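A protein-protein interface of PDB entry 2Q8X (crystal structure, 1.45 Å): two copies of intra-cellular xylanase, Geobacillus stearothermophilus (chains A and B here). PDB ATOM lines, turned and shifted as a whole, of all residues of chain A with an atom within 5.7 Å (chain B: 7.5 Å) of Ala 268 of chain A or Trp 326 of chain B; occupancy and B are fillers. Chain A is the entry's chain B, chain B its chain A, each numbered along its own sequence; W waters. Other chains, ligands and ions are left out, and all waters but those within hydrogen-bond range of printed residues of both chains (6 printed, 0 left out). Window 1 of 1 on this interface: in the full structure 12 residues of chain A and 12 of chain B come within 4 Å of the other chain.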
ATOM      1  N   MET A 263       3.851  -6.974  -9.148  1.00  0.00           N
ATOM      2  CA  MET A 263       4.971  -7.771  -8.625  1.00  0.00           C
ATOM      3  C   MET A 263       4.471  -8.809  -7.592  1.00  0.00           C
ATOM      4  O   MET A 263       4.772  -9.990  -7.731  1.00  0.00           O
ATOM      5  CB  MET A 263       5.863  -6.934  -7.722  1.00  0.00           C
ATOM      6  CG  MET A 263       6.453  -5.744  -8.392  1.00  0.00           C
ATOM      7  SD  MET A 263       8.208  -5.686  -8.418  1.00  0.00           S
ATOM      8  CE  MET A 263       8.708  -4.627  -7.132  1.00  0.00           C
ATOM      9  N   ILE A 264       3.736  -8.225  -6.638  1.00  0.00           N
ATOM     10  CA  ILE A 264       3.211  -9.119  -5.600  1.00  0.00           C
ATOM     11  C   ILE A 264       2.322 -10.194  -6.198  1.00  0.00           C
ATOM     12  O   ILE A 264       2.471 -11.380  -5.808  1.00  0.00           O
ATOM     13  CB  ILE A 264       2.500  -8.318  -4.504  1.00  0.00           C
ATOM     14  CG1 ILE A 264       3.474  -7.505  -3.628  1.00  0.00           C
ATOM     15  CG2 ILE A 264       1.648  -9.222  -3.626  1.00  0.00           C
ATOM     16  CD1 ILE A 264       4.425  -8.381  -2.807  1.00  0.00           C
ATOM     17  N   GLU A 265       1.385  -9.882  -7.082  1.00  0.00           N
ATOM     18  CA  GLU A 265       0.487 -10.885  -7.641  1.00  0.00           C
ATOM     19  C   GLU A 265       1.216 -11.851  -8.570  1.00  0.00           C
ATOM     20  O   GLU A 265       0.967 -13.054  -8.558  1.00  0.00           O
ATOM     21  CB  GLU A 265      -0.631 -10.187  -8.439  1.00  0.00           C
ATOM     22  CG  GLU A 265      -1.565  -9.377  -7.573  1.00  0.00           C
ATOM     23  CD  GLU A 265      -2.496  -8.436  -8.307  1.00  0.00           C
ATOM     24  OE1 GLU A 265      -2.552  -8.454  -9.548  1.00  0.00           O
ATOM     25  OE2 GLU A 265      -3.169  -7.660  -7.580  1.00  0.00           O
ATOM     26  N   ARG A 266       2.157 -11.341  -9.398  1.00  0.00           N
ATOM     27  CA  ARG A 266       2.869 -12.315 -10.227  1.00  0.00           C
ATOM     28  C   ARG A 266       3.744 -13.265  -9.401  1.00  0.00           C
ATOM     29  O   ARG A 266       3.925 -14.452  -9.676  1.00  0.00           O
ATOM     30  CB  ARG A 266       3.806 -11.626 -11.218  1.00  0.00           C
ATOM     31  CG  ARG A 266       4.811 -12.577 -11.852  1.00  0.00           C
ATOM     32  CD  ARG A 266       4.081 -13.647 -12.656  1.00  0.00           C
ATOM     33  NE  ARG A 266       4.975 -14.554 -13.379  1.00  0.00           N
ATOM     34  CZ  ARG A 266       4.638 -15.853 -13.435  1.00  0.00           C
ATOM     35  NH1 ARG A 266       3.514 -16.238 -12.831  1.00  0.00           N
ATOM     36  NH2 ARG A 266       5.432 -16.686 -14.083  1.00  0.00           N
ATOM     37  N   GLN A 267       4.385 -12.735  -8.351  1.00  0.00           N
ATOM     38  CA  GLN A 267       5.212 -13.584  -7.517  1.00  0.00           C
ATOM     39  C   GLN A 267       4.369 -14.674  -6.863  1.00  0.00           C
ATOM     40  O   GLN A 267       4.850 -15.808  -6.660  1.00  0.00           O
ATOM     41  CB  GLN A 267       5.900 -12.739  -6.438  1.00  0.00           C
ATOM     42  CG  GLN A 267       6.755 -13.575  -5.506  1.00  0.00           C
ATOM     43  CD  GLN A 267       7.407 -12.756  -4.406  1.00  0.00           C
ATOM     44  OE1 GLN A 267       6.672 -12.194  -3.570  1.00  0.00           O
ATOM     45  NE2 GLN A 267       8.736 -12.659  -4.433  1.00  0.00           N
ATOM     46  N   ALA A 268       3.143 -14.327  -6.502  1.00  0.00           N
ATOM     47  CA  ALA A 268       2.261 -15.331  -5.863  1.00  0.00           C
ATOM     48  C   ALA A 268       1.953 -16.474  -6.824  1.00  0.00           C
ATOM     49  O   ALA A 268       2.020 -17.653  -6.444  1.00  0.00           O
ATOM     50  CB  ALA A 268       0.968 -14.696  -5.323  1.00  0.00           C
ATOM     51  N   GLU A 269       1.573 -16.091  -8.048  1.00  0.00           N
ATOM     52  CA  GLU A 269       1.296 -17.091  -9.064  1.00  0.00           C
ATOM     53  C   GLU A 269       2.541 -17.921  -9.288  1.00  0.00           C
ATOM     54  O   GLU A 269       2.484 -19.152  -9.318  1.00  0.00           O
ATOM     55  CB  GLU A 269       0.838 -16.419 -10.357  1.00  0.00           C
ATOM     56  CG  GLU A 269       0.566 -17.376 -11.502  1.00  0.00           C
ATOM     57  CD  GLU A 269       0.346 -16.659 -12.809  1.00  0.00           C
ATOM     58  OE1 GLU A 269       1.095 -15.748 -13.248  1.00  0.00           O
ATOM     59  OE2 GLU A 269      -0.668 -17.039 -13.434  1.00  0.00           O
ATOM     60  N   ARG A 270       3.708 -17.290  -9.385  1.00  0.00           N
ATOM     61  CA  ARG A 270       4.971 -18.001  -9.605  1.00  0.00           C
ATOM     62  C   ARG A 270       5.279 -19.057  -8.533  1.00  0.00           C
ATOM     63  O   ARG A 270       5.646 -20.214  -8.825  1.00  0.00           O
ATOM     64  CB  ARG A 270       6.103 -16.975  -9.646  1.00  0.00           C
ATOM     65  CG  ARG A 270       7.525 -17.412  -9.896  1.00  0.00           C
ATOM     66  CD  ARG A 270       7.679 -18.223 -11.182  1.00  0.00           C
ATOM     67  NE  ARG A 270       9.103 -18.217 -11.567  1.00  0.00           N
ATOM     68  CZ  ARG A 270       9.716 -18.952 -12.479  1.00  0.00           C
ATOM     69  NH1 ARG A 270       8.964 -19.837 -13.165  1.00  0.00           N
ATOM     70  NH2 ARG A 270      11.017 -18.843 -12.741  1.00  0.00           N
ATOM     71  N   TYR A 271       5.138 -18.621  -7.274  1.00  0.00           N
ATOM     72  CA  TYR A 271       5.413 -19.526  -6.135  1.00  0.00           C
ATOM     73  C   TYR A 271       4.367 -20.626  -6.089  1.00  0.00           C
ATOM     74  O   TYR A 271       4.738 -21.751  -5.779  1.00  0.00           O
ATOM     75  CB  TYR A 271       5.451 -18.740  -4.843  1.00  0.00           C
ATOM     76  CG  TYR A 271       6.812 -18.343  -4.322  1.00  0.00           C
ATOM     77  CD1 TYR A 271       7.781 -19.313  -3.996  1.00  0.00           C
ATOM     78  CD2 TYR A 271       7.158 -17.009  -4.097  1.00  0.00           C
ATOM     79  CE1 TYR A 271       9.016 -18.928  -3.516  1.00  0.00           C
ATOM     80  CE2 TYR A 271       8.401 -16.621  -3.609  1.00  0.00           C
ATOM     81  CZ  TYR A 271       9.341 -17.599  -3.312  1.00  0.00           C
ATOM     82  OH  TYR A 271      10.590 -17.303  -2.794  1.00  0.00           O
ATOM     83  N   GLY A 272       3.112 -20.329  -6.442  1.00  0.00           N
ATOM     84  CA  GLY A 272       2.127 -21.429  -6.471  1.00  0.00           C
ATOM     85  C   GLY A 272       2.518 -22.423  -7.574  1.00  0.00           C
ATOM     86  O   GLY A 272       2.439 -23.640  -7.369  1.00  0.00           O
ATOM     87  N   GLN A 273       2.942 -21.944  -8.742  1.00  0.00           N
ATOM     88  CA  GLN A 273       3.341 -22.823  -9.846  1.00  0.00           C
ATOM     89  C   GLN A 273       4.538 -23.673  -9.468  1.00  0.00           C
ATOM     90  O   GLN A 273       4.599 -24.862  -9.768  1.00  0.00           O
ATOM     91  CB  GLN A 273       3.673 -21.939 -11.051  1.00  0.00           C
ATOM     92  CG  GLN A 273       2.388 -21.456 -11.771  1.00  0.00           C
ATOM     93  CD  GLN A 273       2.678 -20.268 -12.683  1.00  0.00           C
ATOM     94  OE1 GLN A 273       3.783 -19.703 -12.748  1.00  0.00           O
ATOM     95  NE2 GLN A 273       1.701 -19.784 -13.440  1.00  0.00           N
ATOM     96  N   PRO A 323       0.880 -12.876  -0.306  1.00  0.00           N
ATOM     97  CA  PRO A 323       0.120 -13.687  -1.284  1.00  0.00           C
ATOM     98  C   PRO A 323       0.904 -14.920  -1.710  1.00  0.00           C
ATOM     99  O   PRO A 323       0.346 -16.032  -1.835  1.00  0.00           O
ATOM    100  CB  PRO A 323      -0.091 -12.672  -2.392  1.00  0.00           C
ATOM    101  CG  PRO A 323      -0.361 -11.403  -1.605  1.00  0.00           C
ATOM    102  CD  PRO A 323       0.794 -11.434  -0.623  1.00  0.00           C
ATOM    103  N   ALA A 324       2.213 -14.796  -1.856  1.00  0.00           N
ATOM    104  CA  ALA A 324       3.023 -15.963  -2.219  1.00  0.00           C
ATOM    105  C   ALA A 324       2.919 -17.130  -1.244  1.00  0.00           C
ATOM    106  O   ALA A 324       2.940 -18.297  -1.641  1.00  0.00           O
ATOM    107  CB  ALA A 324       4.499 -15.530  -2.307  1.00  0.00           C
ATOM    108  N   TRP A 326       0.362 -17.880   0.643  1.00  0.00           N
ATOM    109  CA  TRP A 326      -0.945 -18.542   0.510  1.00  0.00           C
ATOM    110  C   TRP A 326      -1.019 -19.355  -0.774  1.00  0.00           C
ATOM    111  O   TRP A 326      -1.557 -20.484  -0.742  1.00  0.00           O
ATOM    112  CB  TRP A 326      -2.077 -17.501   0.616  1.00  0.00           C
ATOM    113  CG  TRP A 326      -2.092 -16.978   2.027  1.00  0.00           C
ATOM    114  CD1 TRP A 326      -1.787 -15.714   2.447  1.00  0.00           C
ATOM    115  CD2 TRP A 326      -2.432 -17.727   3.201  1.00  0.00           C
ATOM    116  NE1 TRP A 326      -1.920 -15.631   3.834  1.00  0.00           N
ATOM    117  CE2 TRP A 326      -2.311 -16.858   4.295  1.00  0.00           C
ATOM    118  CE3 TRP A 326      -2.832 -19.069   3.406  1.00  0.00           C
ATOM    119  CZ2 TRP A 326      -2.571 -17.283   5.589  1.00  0.00           C
ATOM    120  CZ3 TRP A 326      -3.088 -19.467   4.711  1.00  0.00           C
ATOM    121  CH2 TRP A 326      -2.961 -18.582   5.782  1.00  0.00           C
ATOM    122  N   ARG A 327      -0.453 -18.844  -1.858  1.00  0.00           N
ATOM    123  CA  ARG A 327      -0.506 -19.711  -3.033  1.00  0.00           C
ATOM    124  C   ARG A 327       0.408 -20.918  -2.911  1.00  0.00           C
ATOM    125  O   ARG A 327       0.076 -22.024  -3.376  1.00  0.00           O
ATOM    126  CB  ARG A 327      -0.190 -18.936  -4.315  1.00  0.00           C
ATOM    127  CG  ARG A 327      -1.030 -17.685  -4.500  1.00  0.00           C
ATOM    128  CD  ARG A 327      -2.527 -18.051  -4.373  1.00  0.00           C
ATOM    129  NE  ARG A 327      -2.991 -18.887  -5.458  1.00  0.00           N
ATOM    130  CZ  ARG A 327      -3.974 -19.781  -5.393  1.00  0.00           C
ATOM    131  NH1 ARG A 327      -4.639 -19.984  -4.246  1.00  0.00           N
ATOM    132  NH2 ARG A 327      -4.325 -20.493  -6.468  1.00  0.00           N
ATOM    133  N   ALA A 328       1.581 -20.779  -2.285  1.00  0.00           N
ATOM    134  CA  ALA A 328       2.438 -21.954  -2.119  1.00  0.00           C
ATOM    135  C   ALA A 328       1.760 -23.045  -1.306  1.00  0.00           C
ATOM    136  O   ALA A 328       1.844 -24.233  -1.625  1.00  0.00           O
ATOM    137  CB  ALA A 328       3.707 -21.456  -1.433  1.00  0.00           C
ATOM    138  N   SER B   4      -2.586 -11.749 -13.174  1.00  0.00           N
ATOM    139  CA  SER B   4      -2.193 -13.054 -12.693  1.00  0.00           C
ATOM    140  C   SER B   4      -3.068 -13.527 -11.543  1.00  0.00           C
ATOM    141  O   SER B   4      -2.708 -14.530 -10.884  1.00  0.00           O
ATOM    142  CB  SER B   4      -0.743 -13.029 -12.177  1.00  0.00           C
ATOM    143  OG  SER B   4      -0.660 -12.223 -11.008  1.00  0.00           O
ATOM    144  N   LEU B   5      -4.180 -12.824 -11.291  1.00  0.00           N
ATOM    145  CA  LEU B   5      -4.975 -13.234 -10.129  1.00  0.00           C
ATOM    146  C   LEU B   5      -5.833 -14.473 -10.366  1.00  0.00           C
ATOM    147  O   LEU B   5      -6.406 -14.584 -11.449  1.00  0.00           O
ATOM    148  CB  LEU B   5      -5.964 -12.138  -9.695  1.00  0.00           C
ATOM    149  CG  LEU B   5      -5.417 -10.880  -9.049  1.00  0.00           C
ATOM    150  CD1 LEU B   5      -6.576  -9.920  -8.767  1.00  0.00           C
ATOM    151  CD2 LEU B   5      -4.677 -11.163  -7.757  1.00  0.00           C
ATOM    152  N   PRO B   6      -6.002 -15.351  -9.386  1.00  0.00           N
ATOM    153  CA  PRO B   6      -6.960 -16.450  -9.523  1.00  0.00           C
ATOM    154  C   PRO B   6      -8.382 -15.948  -9.719  1.00  0.00           C
ATOM    155  O   PRO B   6      -8.718 -14.880  -9.191  1.00  0.00           O
ATOM    156  CB  PRO B   6      -6.880 -17.175  -8.161  1.00  0.00           C
ATOM    157  CG  PRO B   6      -5.521 -16.831  -7.636  1.00  0.00           C
ATOM    158  CD  PRO B   6      -5.262 -15.411  -8.103  1.00  0.00           C
ATOM    159  N   ALA B 268      -9.052 -11.419   7.284  1.00  0.00           N
ATOM    160  CA  ALA B 268      -8.428 -12.381   6.353  1.00  0.00           C
ATOM    161  C   ALA B 268      -8.475 -13.793   6.950  1.00  0.00           C
ATOM    162  O   ALA B 268      -8.854 -14.768   6.301  1.00  0.00           O
ATOM    163  CB  ALA B 268      -6.986 -11.968   6.003  1.00  0.00           C
ATOM    164  N   GLY B 272     -10.537 -17.028   5.541  1.00  0.00           N
ATOM    165  CA  GLY B 272      -9.909 -18.324   5.233  1.00  0.00           C
ATOM    166  C   GLY B 272     -10.600 -19.471   5.965  1.00  0.00           C
ATOM    167  O   GLY B 272     -10.809 -20.573   5.453  1.00  0.00           O
ATOM    168  N   LEU B 314     -14.147  -9.209  -0.331  1.00  0.00           N
ATOM    169  CA  LEU B 314     -12.783  -9.696  -0.633  1.00  0.00           C
ATOM    170  C   LEU B 314     -11.970  -8.663  -1.423  1.00  0.00           C
ATOM    171  O   LEU B 314     -10.731  -8.843  -1.472  1.00  0.00           O
ATOM    172  CB  LEU B 314     -12.834 -10.979  -1.449  1.00  0.00           C
ATOM    173  CG  LEU B 314     -13.486 -12.212  -0.810  1.00  0.00           C
ATOM    174  CD1 LEU B 314     -13.273 -13.427  -1.716  1.00  0.00           C
ATOM    175  CD2 LEU B 314     -12.959 -12.472   0.592  1.00  0.00           C
ATOM    176  N   LYS B 320      -9.127  -3.870  -5.751  1.00  0.00           N
ATOM    177  CA  LYS B 320      -7.939  -4.725  -5.639  1.00  0.00           C
ATOM    178  C   LYS B 320      -8.122  -5.812  -4.585  1.00  0.00           C
ATOM    179  O   LYS B 320      -8.808  -5.546  -3.588  1.00  0.00           O
ATOM    180  CB  LYS B 320      -6.725  -3.830  -5.292  1.00  0.00           C
ATOM    181  CG  LYS B 320      -6.505  -2.783  -6.407  1.00  0.00           C
ATOM    182  CD  LYS B 320      -5.881  -3.588  -7.560  1.00  0.00           C
ATOM    183  CE  LYS B 320      -4.846  -4.526  -6.886  1.00  0.00           C
ATOM    184  NZ  LYS B 320      -4.339  -5.490  -7.882  1.00  0.00           N
ATOM    185  N   PRO B 321      -7.545  -7.004  -4.697  1.00  0.00           N
ATOM    186  CA  PRO B 321      -7.747  -8.016  -3.658  1.00  0.00           C
ATOM    187  C   PRO B 321      -7.194  -7.595  -2.309  1.00  0.00           C
ATOM    188  O   PRO B 321      -6.102  -7.007  -2.238  1.00  0.00           O
ATOM    189  CB  PRO B 321      -6.924  -9.207  -4.136  1.00  0.00           C
ATOM    190  CG  PRO B 321      -5.943  -8.599  -5.100  1.00  0.00           C
ATOM    191  CD  PRO B 321      -6.665  -7.472  -5.794  1.00  0.00           C
ATOM    192  N   LYS B 322      -7.912  -7.898  -1.250  1.00  0.00           N
ATOM    193  CA  LYS B 322      -7.508  -7.670   0.127  1.00  0.00           C
ATOM    194  C   LYS B 322      -6.831  -8.914   0.671  1.00  0.00           C
ATOM    195  O   LYS B 322      -6.870  -9.963   0.008  1.00  0.00           O
ATOM    196  CB  LYS B 322      -8.782  -7.366   0.954  1.00  0.00           C
ATOM    197  CG  LYS B 322      -9.391  -5.999   0.606  1.00  0.00           C
ATOM    198  CD  LYS B 322     -10.829  -5.863   1.096  1.00  0.00           C
ATOM    199  CE  LYS B 322     -10.996  -5.960   2.600  1.00  0.00           C
ATOM    200  NZ  LYS B 322     -12.449  -5.941   2.957  1.00  0.00           N
ATOM    201  N   PRO B 323      -6.175  -8.846   1.816  1.00  0.00           N
ATOM    202  CA  PRO B 323      -5.601 -10.050   2.465  1.00  0.00           C
ATOM    203  C   PRO B 323      -6.619 -11.187   2.552  1.00  0.00           C
ATOM    204  O   PRO B 323      -6.304 -12.375   2.343  1.00  0.00           O
ATOM    205  CB  PRO B 323      -5.233  -9.483   3.826  1.00  0.00           C
ATOM    206  CG  PRO B 323      -4.759  -8.080   3.448  1.00  0.00           C
ATOM    207  CD  PRO B 323      -5.912  -7.595   2.571  1.00  0.00           C
ATOM    208  N   ALA B 324      -7.882 -10.852   2.808  1.00  0.00           N
ATOM    209  CA  ALA B 324      -8.930 -11.882   2.819  1.00  0.00           C
ATOM    210  C   ALA B 324      -9.044 -12.664   1.521  1.00  0.00           C
ATOM    211  O   ALA B 324      -9.356 -13.863   1.487  1.00  0.00           O
ATOM    212  CB  ALA B 324     -10.277 -11.204   3.092  1.00  0.00           C
ATOM    213  N   PHE B 325      -8.833 -12.032   0.366  1.00  0.00           N
ATOM    214  CA  PHE B 325      -8.926 -12.745  -0.900  1.00  0.00           C
ATOM    215  C   PHE B 325      -7.951 -13.918  -0.934  1.00  0.00           C
ATOM    216  O   PHE B 325      -8.293 -15.026  -1.368  1.00  0.00           O
ATOM    217  CB  PHE B 325      -8.624 -11.757  -2.052  1.00  0.00           C
ATOM    218  CG  PHE B 325      -8.452 -12.413  -3.418  1.00  0.00           C
ATOM    219  CD1 PHE B 325      -9.582 -12.588  -4.233  1.00  0.00           C
ATOM    220  CD2 PHE B 325      -7.219 -12.799  -3.923  1.00  0.00           C
ATOM    221  CE1 PHE B 325      -9.420 -13.157  -5.479  1.00  0.00           C
ATOM    222  CE2 PHE B 325      -7.082 -13.406  -5.150  1.00  0.00           C
ATOM    223  CZ  PHE B 325      -8.182 -13.593  -5.957  1.00  0.00           C
ATOM    224  N   TRP B 326      -6.685 -13.621  -0.542  1.00  0.00           N
ATOM    225  CA  TRP B 326      -5.634 -14.634  -0.703  1.00  0.00           C
ATOM    226  C   TRP B 326      -5.871 -15.812   0.220  1.00  0.00           C
ATOM    227  O   TRP B 326      -5.592 -16.960  -0.138  1.00  0.00           O
ATOM    228  CB  TRP B 326      -4.307 -13.960  -0.381  1.00  0.00           C
ATOM    229  CG  TRP B 326      -4.010 -12.865  -1.399  1.00  0.00           C
ATOM    230  CD1 TRP B 326      -4.107 -11.506  -1.212  1.00  0.00           C
ATOM    231  CD2 TRP B 326      -3.583 -13.065  -2.751  1.00  0.00           C
ATOM    232  NE1 TRP B 326      -3.758 -10.844  -2.372  1.00  0.00           N
ATOM    233  CE2 TRP B 326      -3.431 -11.788  -3.329  1.00  0.00           C
ATOM    234  CE3 TRP B 326      -3.311 -14.209  -3.523  1.00  0.00           C
ATOM    235  CZ2 TRP B 326      -3.014 -11.635  -4.654  1.00  0.00           C
ATOM    236  CZ3 TRP B 326      -2.895 -14.057  -4.844  1.00  0.00           C
ATOM    237  CH2 TRP B 326      -2.755 -12.761  -5.390  1.00  0.00           C
ATOM    238  N   ARG B 327      -6.409 -15.552   1.418  1.00  0.00           N
ATOM    239  CA  ARG B 327      -6.704 -16.703   2.277  1.00  0.00           C
ATOM    240  C   ARG B 327      -7.904 -17.465   1.773  1.00  0.00           C
ATOM    241  O   ARG B 327      -7.907 -18.681   1.808  1.00  0.00           O
ATOM    242  CB  ARG B 327      -7.038 -16.265   3.708  1.00  0.00           C
ATOM    243  CG  ARG B 327      -5.821 -15.700   4.417  1.00  0.00           C
ATOM    244  CD  ARG B 327      -5.692 -16.199   5.850  1.00  0.00           C
ATOM    245  NE  ARG B 327      -4.732 -15.343   6.563  1.00  0.00           N
ATOM    246  CZ  ARG B 327      -4.336 -15.593   7.798  1.00  0.00           C
ATOM    247  NH1 ARG B 327      -4.811 -16.661   8.423  1.00  0.00           N
ATOM    248  NH2 ARG B 327      -3.454 -14.793   8.410  1.00  0.00           N
ATOM    249  N   ALA B 328      -8.936 -16.754   1.281  1.00  0.00           N
ATOM    250  CA  ALA B 328     -10.139 -17.445   0.785  1.00  0.00           C
ATOM    251  C   ALA B 328      -9.791 -18.357  -0.382  1.00  0.00           C
ATOM    252  O   ALA B 328     -10.256 -19.494  -0.391  1.00  0.00           O
ATOM    253  CB  ALA B 328     -11.212 -16.420   0.409  1.00  0.00           C
ATOM    254  N   VAL B 329      -8.974 -17.880  -1.340  1.00  0.00           N
ATOM    255  CA  VAL B 329      -8.740 -18.714  -2.505  1.00  0.00           C
ATOM    256  C   VAL B 329      -7.706 -19.796  -2.257  1.00  0.00           C
ATOM    257  O   VAL B 329      -7.444 -20.609  -3.146  1.00  0.00           O
ATOM    258  CB  VAL B 329      -8.320 -17.892  -3.748  1.00  0.00           C
ATOM    259  CG1 VAL B 329      -9.470 -17.016  -4.179  1.00  0.00           C
ATOM    260  CG2 VAL B 329      -7.046 -17.080  -3.535  1.00  0.00           C
ATOM    261  N   SER B 330      -7.102 -19.846  -1.089  1.00  0.00           N
ATOM    262  CA  SER B 330      -5.997 -20.823  -0.941  1.00  0.00           C
ATOM    263  C   SER B 330      -6.345 -22.038  -0.083  1.00  0.00           C
ATOM    264  O   SER B 330      -5.436 -22.819   0.205  1.00  0.00           O
ATOM    265  CB  SER B 330      -4.734 -20.068  -0.497  1.00  0.00           C
ATOM    266  OG  SER B 330      -4.411 -19.087  -1.500  1.00  0.00           O
ATOM    267  N   VAL B 331      -7.622 -22.172   0.254  1.00  0.00           N
ATOM    268  CA  VAL B 331      -8.093 -23.296   1.064  1.00  0.00           C
ATOM    269  C   VAL B 331      -8.125 -24.628   0.322  1.00  0.00           C
ATOM    270  O   VAL B 331      -8.292 -25.704   0.913  1.00  0.00           O
ATOM    271  CB  VAL B 331      -9.520 -23.065   1.637  1.00  0.00           C
ATOM    272  CG1 VAL B 331      -9.527 -21.818   2.526  1.00  0.00           C
ATOM    273  CG2 VAL B 331     -10.563 -22.974   0.538  1.00  0.00           C
ATOM    274  OXT VAL B 331      -7.935 -24.731  -1.208  1.00  0.00           O
HETATM  275  O   HOH W   1      -2.884 -12.941   5.850  1.00  0.00           O
HETATM  276  O   HOH W   2      -3.514 -12.763   2.960  1.00  0.00           O
HETATM  277  O   HOH W   3      -1.653 -14.346  -8.406  1.00  0.00           O
HETATM  278  O   HOH W   4      -1.459  -9.564 -11.805  1.00  0.00           O
HETATM  279  O   HOH W   5      -6.198 -22.473  -5.798  1.00  0.00           O
HETATM  280  O   HOH W   6      -2.065  -5.850 -10.406  1.00  0.00           O
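NH1 of Arg 327 of chain A is in hydrogen-bond range of OG of Ser 330 of chain B (2.9 Å).
OG of Ser 330 of chain B lies close to O of Trp 326 of chain A.
The side-chain hydroxyl (OG) of Ser 4 of chain B lies within hydrogen-bond range of the backbone carbonyl oxygen (O) of Glu 265 of chain A (3.1 Å).
N of Arg 266 of chain A lies within hydrogen-bond range of OG of Ser 4 of chain B (3.4 Å).
The backbone carbonyl oxygen of Val 329 of chain B lies within hydrogen-bond range of the guanidinium group of Arg 327 of chain A, at 3.1 Å.
The side-chain carboxylate of Glu 265 of chain A lies within salt-bridge range of the side-chain amino group of Lys 320 of chain B, at 2.5 Å.
Of the printed residues of chain B, Glu 265 of chain A touches Ser 4, Leu 5, Lys 320, Pro 321 and Trp 326.
Of chain B, only Trp 326 comes within 4 Å of Ala 268 of chain A.
Of the printed residues of chain B, Pro 323 of chain A touches Trp 326 (3.5 Å).
Of the printed residues of chain A, Lys 320 of chain B touches Glu 265.
Printed residues of chain A within 4 Å of Pro 321 of chain B: Glu 265.
Of the printed residues of chain A, Trp 326 of chain B touches Glu 265 (3.96 Å), Ala 268 (3.9 Å), Pro 323 (3.5 Å) and Trp 326 (3.6 Å).
The nearest residue of chain B that does not touch Ala 268 of chain A is Ser 4 of chain B (6.3 Å).
The nearest printed residue of chain A that does not touch Trp 326 of chain B is Arg 327 of chain A (4.01 Å).
Ala 268 of chain A touches Trp 326 of chain B, but with the chains exchanged Trp 326 of chain A does not touch Ala 268 of chain B (6.6 Å).
Pro 323 of chain A touches Trp 326 of chain B, but with the chains exchanged Trp 326 of chain A does not touch Pro 323 of chain B (5.6 Å).
Trp 326 of chain B touches its own counterpart, Trp 326 of chain A.
Trp 326 of chain A touches Arg 327 of chain B, but with the chains exchanged Arg 327 of chain A does not touch Trp 326 of chain B (4.01 Å).
7 positions are printed for both chains.
OE1 of Glu 269 of chain A is in salt-bridge range of NH1 of Arg 266 of chain A, at 2.5 Å.
The guanidinium group of Arg 266 of chain A sits at hydrogen-bond distance from the side-chain amide oxygen of Gln 273 of chain A (3.5 Å).
The backbone carbonyl oxygen (O) of Trp 326 of chain B lies within hydrogen-bond range of the side-chain hydroxyl (OG) of Ser 330 of chain B (2.8 Å).
Leu 5 of chain B touches Glu 265 of chain A (CD2 to CD, 3.5 Å).
Glu 265 of chain A touches Pro 321 of chain B.
CZ2 of Trp 326 of chain B touches CG of Glu 265 of chain A (3.96 Å).
Trp 326 of chain B touches Ala 268 of chain A.
OE1 of Glu 269 of chain A touches CB of Ser 4 of chain B, at 3.5 Å.
CG of Pro 323 of chain A touches NE1 of Trp 326 of chain B, at 3.5 Å.
Trp 326 of chain A touches Trp 326 of chain B.
CZ2 of Trp 326 of chain A touches NE of Arg 327 of chain B (3.1 Å).
CG of Pro 6 of chain B touches NE of Arg 327 of chain A, 3.9 Å away.
Water W3 lies within hydrogen-bond range of O of Ser 4 of chain B and O of Glu 265 of chain A.
Water W4 lies within hydrogen-bond range of the side-chain carboxylate of Glu 265 of chain A (2.7 Å) and the backbone NH of Ser 4 of chain B (2.8 Å).
Water W6 bridges OE1 of Glu 265 of chain A (2.8 Å) and NZ of Lys 320 of chain B (3.4 Å).
Water W5 lies within hydrogen-bond range of NH2 of Arg 327 of chain A (2.8 Å) and O of Val 329 of chain B (3.5 Å).
Water W2 bridges O of Pro 323 of chain B and NE1 of Trp 326 of chain A.
Water W1 lies within hydrogen-bond range of NE of Arg 327 of chain B (3.1 Å) and NE1 of Trp 326 of chain A (3.5 Å).
Of the 16 printed residues of chain A, 7 touch a printed residue of chain B.
Hydrophobic or aromatic side chains of chain A that line the printed part of chain B: Ala 268, Pro 323 and Trp 326.
Along chain A the printed residues that touch a printed residue of chain B span positions 265 to 327.
Of the 18 printed residues of chain B, 9 touch a printed residue of chain A.
Hydrophobic or aromatic side chains of chain B that line the printed part of chain A: Leu 5, Pro 6, Pro 321, Trp 326 and Val 329.
Among the printed residues, 15 pairs touch across the chains.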
